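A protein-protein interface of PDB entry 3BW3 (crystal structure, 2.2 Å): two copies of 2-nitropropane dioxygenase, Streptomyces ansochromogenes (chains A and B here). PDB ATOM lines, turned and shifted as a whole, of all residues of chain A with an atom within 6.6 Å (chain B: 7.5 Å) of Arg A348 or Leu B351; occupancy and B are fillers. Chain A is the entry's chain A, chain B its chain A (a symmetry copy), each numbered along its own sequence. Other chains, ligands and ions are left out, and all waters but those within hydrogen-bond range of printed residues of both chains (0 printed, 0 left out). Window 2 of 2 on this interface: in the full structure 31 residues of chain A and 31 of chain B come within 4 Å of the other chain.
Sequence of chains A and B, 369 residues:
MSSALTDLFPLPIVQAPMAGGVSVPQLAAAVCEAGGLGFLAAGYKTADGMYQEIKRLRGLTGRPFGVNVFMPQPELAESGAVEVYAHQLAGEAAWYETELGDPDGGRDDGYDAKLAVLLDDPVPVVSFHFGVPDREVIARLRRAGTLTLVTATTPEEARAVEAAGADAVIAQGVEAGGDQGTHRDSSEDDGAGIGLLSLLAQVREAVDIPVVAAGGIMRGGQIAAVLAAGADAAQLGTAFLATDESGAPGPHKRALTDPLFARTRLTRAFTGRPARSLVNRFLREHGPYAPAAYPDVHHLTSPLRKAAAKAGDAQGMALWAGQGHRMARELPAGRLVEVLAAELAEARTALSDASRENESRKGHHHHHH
NH1 of Arg A348 is in hydrogen-bond range of O of Leu B351 (2.8 Å).
The backbone carbonyl oxygen of Leu A351 sits at hydrogen-bond distance from the guanidinium group of Arg B348, 2.8 Å away.
Leu B351 touches Ala A224 (CD2 to O, 3.8 Å).
Ala A225 touches Ala B228.
CB of Leu A227 touches CD2 of Leu B351, at 3.9 Å.
O of Ala A228 touches CB of Ala B347 (3.9 Å).
CB of Ala A347 touches O of Ala B228, 3.9 Å away.
CD2 of Leu A351 touches O of Ala B224 (3.8 Å).
Of the printed residues of chain B, Ala A225 touches Ala B228.
Of chain B, only Leu B351 comes within 4 Å of Arg A348.
Printed residues of chain A within 4 Å of Ala B347: Ala A228.
Of the printed residues of chain A, Arg B348 touches Leu A351.
Of chain A, only Ala A224, Leu A227 and Arg A348 come within 4 Å of Leu B351.
The nearest residue of chain B that does not touch Arg A348 is Ala B350 (5.0 Å).
The nearest residue of chain A that does not touch Leu B351 is Ala A228 (4.1 Å).
The nearest printed residue of chain B that does not touch Ala A228 is Ala B224 (4.1 Å).
Of the 15 printed residues of chain A, 7 touch a printed residue of chain B.
Of the 9 printed residues of chain B, 5 touch a printed residue of chain A.
Ala A224 touches Leu B351, and with the chains exchanged Leu A351 touches Ala B224.
Ala A228 touches Ala B347, and with the chains exchanged Ala A347 touches Ala B228.
Arg A348 touches Leu B351, and with the chains exchanged Leu A351 touches Arg B348.
Positions printed for both chains: 224, 228, 345, 346, 347, 348, 349, 350 and 351.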
ATOM      1  N   PRO A  12     -13.556  15.873  -7.584  1.00  0.00           N
ATOM      2  CA  PRO A  12     -12.652  16.506  -6.619  1.00  0.00           C
ATOM      3  C   PRO A  12     -11.217  16.516  -7.131  1.00  0.00           C
ATOM      4  O   PRO A  12     -10.276  16.192  -6.404  1.00  0.00           O
ATOM      5  CB  PRO A  12     -12.816  15.636  -5.385  1.00  0.00           C
ATOM      6  CG  PRO A  12     -12.998  14.266  -5.985  1.00  0.00           C
ATOM      7  CD  PRO A  12     -13.970  14.537  -7.116  1.00  0.00           C
ATOM      8  N   ILE A 223      -6.203  10.053  -4.180  1.00  0.00           N
ATOM      9  CA  ILE A 223      -7.207  11.103  -4.088  1.00  0.00           C
ATOM     10  C   ILE A 223      -8.200  10.687  -3.003  1.00  0.00           C
ATOM     11  O   ILE A 223      -8.662  11.517  -2.224  1.00  0.00           O
ATOM     12  CB  ILE A 223      -7.969  11.303  -5.415  1.00  0.00           C
ATOM     13  CG1 ILE A 223      -7.008  11.803  -6.502  1.00  0.00           C
ATOM     14  CG2 ILE A 223      -9.111  12.307  -5.204  1.00  0.00           C
ATOM     15  CD1 ILE A 223      -7.656  12.011  -7.862  1.00  0.00           C
ATOM     16  N   ALA A 224      -8.521   9.396  -2.957  1.00  0.00           N
ATOM     17  CA  ALA A 224      -9.441   8.874  -1.949  1.00  0.00           C
ATOM     18  C   ALA A 224      -8.791   9.005  -0.577  1.00  0.00           C
ATOM     19  O   ALA A 224      -9.466   9.252   0.427  1.00  0.00           O
ATOM     20  CB  ALA A 224      -9.751   7.419  -2.230  1.00  0.00           C
ATOM     21  N   ALA A 225      -7.473   8.834  -0.542  1.00  0.00           N
ATOM     22  CA  ALA A 225      -6.727   8.937   0.699  1.00  0.00           C
ATOM     23  C   ALA A 225      -6.846  10.326   1.312  1.00  0.00           C
ATOM     24  O   ALA A 225      -7.205  10.460   2.483  1.00  0.00           O
ATOM     25  CB  ALA A 225      -5.262   8.596   0.461  1.00  0.00           C
ATOM     26  N   LEU A 227      -9.038  12.637   0.688  1.00  0.00           N
ATOM     27  CA  LEU A 227     -10.430  12.955   0.997  1.00  0.00           C
ATOM     28  C   LEU A 227     -10.784  12.345   2.354  1.00  0.00           C
ATOM     29  O   LEU A 227     -11.477  12.959   3.169  1.00  0.00           O
ATOM     30  CB  LEU A 227     -11.374  12.394  -0.076  1.00  0.00           C
ATOM     31  CG  LEU A 227     -11.315  12.995  -1.487  1.00  0.00           C
ATOM     32  CD1 LEU A 227     -12.316  12.283  -2.391  1.00  0.00           C
ATOM     33  CD2 LEU A 227     -11.620  14.479  -1.428  1.00  0.00           C
ATOM     34  N   ALA A 228     -10.301  11.130   2.585  1.00  0.00           N
ATOM     35  CA  ALA A 228     -10.553  10.431   3.837  1.00  0.00           C
ATOM     36  C   ALA A 228      -9.893  11.157   5.003  1.00  0.00           C
ATOM     37  O   ALA A 228     -10.368  11.083   6.132  1.00  0.00           O
ATOM     38  CB  ALA A 228     -10.025   8.997   3.749  1.00  0.00           C
ATOM     39  N   GLU A 343     -10.238   5.130 -10.704  1.00  0.00           N
ATOM     40  CA  GLU A 343      -9.401   4.666  -9.604  1.00  0.00           C
ATOM     41  C   GLU A 343      -9.977   5.156  -8.281  1.00  0.00           C
ATOM     42  O   GLU A 343      -9.968   4.437  -7.281  1.00  0.00           O
ATOM     43  CB  GLU A 343      -7.969   5.166  -9.793  1.00  0.00           C
ATOM     44  CG  GLU A 343      -7.233   4.462 -10.932  1.00  0.00           C
ATOM     45  CD  GLU A 343      -5.896   5.093 -11.256  1.00  0.00           C
ATOM     46  OE1 GLU A 343      -5.107   4.464 -11.991  1.00  0.00           O
ATOM     47  OE2 GLU A 343      -5.635   6.221 -10.787  1.00  0.00           O
ATOM     48  N   LEU A 344     -10.489   6.381  -8.289  1.00  0.00           N
ATOM     49  CA  LEU A 344     -11.102   6.969  -7.104  1.00  0.00           C
ATOM     50  C   LEU A 344     -12.301   6.121  -6.669  1.00  0.00           C
ATOM     51  O   LEU A 344     -12.380   5.683  -5.520  1.00  0.00           O
ATOM     52  CB  LEU A 344     -11.562   8.397  -7.412  1.00  0.00           C
ATOM     53  CG  LEU A 344     -12.428   9.126  -6.382  1.00  0.00           C
ATOM     54  CD1 LEU A 344     -11.702   9.192  -5.054  1.00  0.00           C
ATOM     55  CD2 LEU A 344     -12.753  10.525  -6.891  1.00  0.00           C
ATOM     56  N   ALA A 345     -13.226   5.888  -7.597  1.00  0.00           N
ATOM     57  CA  ALA A 345     -14.418   5.095  -7.315  1.00  0.00           C
ATOM     58  C   ALA A 345     -14.023   3.722  -6.794  1.00  0.00           C
ATOM     59  O   ALA A 345     -14.558   3.244  -5.801  1.00  0.00           O
ATOM     60  CB  ALA A 345     -15.264   4.952  -8.583  1.00  0.00           C
ATOM     61  N   GLU A 346     -13.075   3.091  -7.474  1.00  0.00           N
ATOM     62  CA  GLU A 346     -12.603   1.775  -7.074  1.00  0.00           C
ATOM     63  C   GLU A 346     -12.081   1.776  -5.635  1.00  0.00           C
ATOM     64  O   GLU A 346     -12.307   0.824  -4.891  1.00  0.00           O
ATOM     65  CB  GLU A 346     -11.503   1.311  -8.027  1.00  0.00           C
ATOM     66  CG  GLU A 346     -10.726   0.113  -7.529  1.00  0.00           C
ATOM     67  CD  GLU A 346      -9.607  -0.280  -8.465  1.00  0.00           C
ATOM     68  OE1 GLU A 346      -8.808   0.609  -8.841  1.00  0.00           O
ATOM     69  OE2 GLU A 346      -9.521  -1.477  -8.819  1.00  0.00           O
ATOM     70  N   ALA A 347     -11.390   2.845  -5.245  1.00  0.00           N
ATOM     71  CA  ALA A 347     -10.841   2.948  -3.895  1.00  0.00           C
ATOM     72  C   ALA A 347     -11.927   3.199  -2.854  1.00  0.00           C
ATOM     73  O   ALA A 347     -11.848   2.682  -1.745  1.00  0.00           O
ATOM     74  CB  ALA A 347      -9.791   4.047  -3.836  1.00  0.00           C
ATOM     75  N   ARG A 348     -12.932   3.999  -3.201  1.00  0.00           N
ATOM     76  CA  ARG A 348     -14.032   4.277  -2.275  1.00  0.00           C
ATOM     77  C   ARG A 348     -14.728   2.962  -1.956  1.00  0.00           C
ATOM     78  O   ARG A 348     -14.955   2.627  -0.797  1.00  0.00           O
ATOM     79  CB  ARG A 348     -15.069   5.216  -2.901  1.00  0.00           C
ATOM     80  CG  ARG A 348     -14.686   6.679  -3.020  1.00  0.00           C
ATOM     81  CD  ARG A 348     -15.832   7.421  -3.710  1.00  0.00           C
ATOM     82  NE  ARG A 348     -15.564   8.836  -3.951  1.00  0.00           N
ATOM     83  CZ  ARG A 348     -15.658   9.788  -3.031  1.00  0.00           C
ATOM     84  NH1 ARG A 348     -16.015   9.487  -1.788  1.00  0.00           N
ATOM     85  NH2 ARG A 348     -15.407  11.049  -3.357  1.00  0.00           N
ATOM     86  N   THR A 349     -15.076   2.227  -3.007  1.00  0.00           N
ATOM     87  CA  THR A 349     -15.753   0.946  -2.860  1.00  0.00           C
ATOM     88  C   THR A 349     -14.996   0.038  -1.903  1.00  0.00           C
ATOM     89  O   THR A 349     -15.573  -0.481  -0.948  1.00  0.00           O
ATOM     90  CB  THR A 349     -15.908   0.249  -4.230  1.00  0.00           C
ATOM     91  OG1 THR A 349     -16.774   1.031  -5.060  1.00  0.00           O
ATOM     92  CG2 THR A 349     -16.499  -1.143  -4.068  1.00  0.00           C
ATOM     93  N   ALA A 350     -13.703  -0.143  -2.153  1.00  0.00           N
ATOM     94  CA  ALA A 350     -12.869  -0.993  -1.310  1.00  0.00           C
ATOM     95  C   ALA A 350     -12.861  -0.526   0.141  1.00  0.00           C
ATOM     96  O   ALA A 350     -12.980  -1.332   1.060  1.00  0.00           O
ATOM     97  CB  ALA A 350     -11.450  -1.024  -1.850  1.00  0.00           C
ATOM     98  N   LEU A 351     -12.722   0.781   0.339  1.00  0.00           N
ATOM     99  CA  LEU A 351     -12.690   1.368   1.675  1.00  0.00           C
ATOM    100  C   LEU A 351     -14.066   1.277   2.339  1.00  0.00           C
ATOM    101  O   LEU A 351     -14.186   1.350   3.562  1.00  0.00           O
ATOM    102  CB  LEU A 351     -12.234   2.831   1.573  1.00  0.00           C
ATOM    103  CG  LEU A 351     -11.789   3.629   2.803  1.00  0.00           C
ATOM    104  CD1 LEU A 351     -12.992   4.036   3.634  1.00  0.00           C
ATOM    105  CD2 LEU A 351     -10.795   2.805   3.616  1.00  0.00           C
ATOM    106  N   ALA B 224      -7.672   5.738   7.713  1.00  0.00           N
ATOM    107  CA  ALA B 224      -8.568   5.490   6.585  1.00  0.00           C
ATOM    108  C   ALA B 224      -7.873   5.929   5.301  1.00  0.00           C
ATOM    109  O   ALA B 224      -8.049   5.322   4.241  1.00  0.00           O
ATOM    110  CB  ALA B 224      -9.855   6.267   6.761  1.00  0.00           C
ATOM    111  N   ALA B 228      -7.037   3.518   2.095  1.00  0.00           N
ATOM    112  CA  ALA B 228      -7.572   3.884   0.792  1.00  0.00           C
ATOM    113  C   ALA B 228      -6.467   3.906  -0.258  1.00  0.00           C
ATOM    114  O   ALA B 228      -6.722   3.671  -1.436  1.00  0.00           O
ATOM    115  CB  ALA B 228      -8.247   5.255   0.869  1.00  0.00           C
ATOM    116  N   ALA B 345     -13.942   4.587  11.629  1.00  0.00           N
ATOM    117  CA  ALA B 345     -15.300   4.297  11.180  1.00  0.00           C
ATOM    118  C   ALA B 345     -15.954   5.560  10.641  1.00  0.00           C
ATOM    119  O   ALA B 345     -16.554   5.556   9.572  1.00  0.00           O
ATOM    120  CB  ALA B 345     -16.126   3.730  12.336  1.00  0.00           C
ATOM    121  N   GLU B 346     -15.829   6.646  11.391  1.00  0.00           N
ATOM    122  CA  GLU B 346     -16.403   7.919  10.985  1.00  0.00           C
ATOM    123  C   GLU B 346     -15.883   8.360   9.614  1.00  0.00           C
ATOM    124  O   GLU B 346     -16.638   8.896   8.805  1.00  0.00           O
ATOM    125  CB  GLU B 346     -16.085   8.985  12.031  1.00  0.00           C
ATOM    126  CG  GLU B 346     -16.353  10.399  11.566  1.00  0.00           C
ATOM    127  CD  GLU B 346     -15.969  11.430  12.602  1.00  0.00           C
ATOM    128  OE1 GLU B 346     -14.824  11.367  13.106  1.00  0.00           O
ATOM    129  OE2 GLU B 346     -16.808  12.308  12.906  1.00  0.00           O
ATOM    130  N   ALA B 347     -14.598   8.130   9.356  1.00  0.00           N
ATOM    131  CA  ALA B 347     -13.996   8.517   8.081  1.00  0.00           C
ATOM    132  C   ALA B 347     -14.447   7.613   6.938  1.00  0.00           C
ATOM    133  O   ALA B 347     -14.640   8.082   5.821  1.00  0.00           O
ATOM    134  CB  ALA B 347     -12.479   8.507   8.191  1.00  0.00           C
ATOM    135  N   ARG B 348     -14.604   6.319   7.208  1.00  0.00           N
ATOM    136  CA  ARG B 348     -15.059   5.381   6.180  1.00  0.00           C
ATOM    137  C   ARG B 348     -16.445   5.812   5.724  1.00  0.00           C
ATOM    138  O   ARG B 348     -16.712   5.937   4.532  1.00  0.00           O
ATOM    139  CB  ARG B 348     -15.169   3.955   6.730  1.00  0.00           C
ATOM    140  CG  ARG B 348     -13.870   3.206   6.960  1.00  0.00           C
ATOM    141  CD  ARG B 348     -14.203   1.835   7.552  1.00  0.00           C
ATOM    142  NE  ARG B 348     -13.031   1.033   7.889  1.00  0.00           N
ATOM    143  CZ  ARG B 348     -12.311   0.346   7.009  1.00  0.00           C
ATOM    144  NH1 ARG B 348     -12.635   0.358   5.722  1.00  0.00           N
ATOM    145  NH2 ARG B 348     -11.271  -0.367   7.421  1.00  0.00           N
ATOM    146  N   THR B 349     -17.328   6.024   6.693  1.00  0.00           N
ATOM    147  CA  THR B 349     -18.696   6.436   6.411  1.00  0.00           C
ATOM    148  C   THR B 349     -18.720   7.656   5.503  1.00  0.00           C
ATOM    149  O   THR B 349     -19.382   7.649   4.465  1.00  0.00           O
ATOM    150  CB  THR B 349     -19.455   6.746   7.721  1.00  0.00           C
ATOM    151  OG1 THR B 349     -19.583   5.542   8.486  1.00  0.00           O
ATOM    152  CG2 THR B 349     -20.842   7.298   7.429  1.00  0.00           C
ATOM    153  N   ALA B 350     -17.987   8.698   5.888  1.00  0.00           N
ATOM    154  CA  ALA B 350     -17.929   9.926   5.102  1.00  0.00           C
ATOM    155  C   ALA B 350     -17.426   9.675   3.685  1.00  0.00           C
ATOM    156  O   ALA B 350     -17.984  10.195   2.721  1.00  0.00           O
ATOM    157  CB  ALA B 350     -17.035  10.940   5.795  1.00  0.00           C
ATOM    158  N   LEU B 351     -16.373   8.876   3.567  1.00  0.00           N
ATOM    159  CA  LEU B 351     -15.781   8.554   2.271  1.00  0.00           C
ATOM    160  C   LEU B 351     -16.719   7.662   1.454  1.00  0.00           C
ATOM    161  O   LEU B 351     -16.613   7.583   0.230  1.00  0.00           O
ATOM    162  CB  LEU B 351     -14.430   7.858   2.493  1.00  0.00           C
ATOM    163  CG  LEU B 351     -13.414   7.680   1.358  1.00  0.00           C
ATOM    164  CD1 LEU B 351     -13.858   6.574   0.419  1.00  0.00           C
ATOM    165  CD2 LEU B 351     -13.230   9.004   0.623  1.00  0.00           C
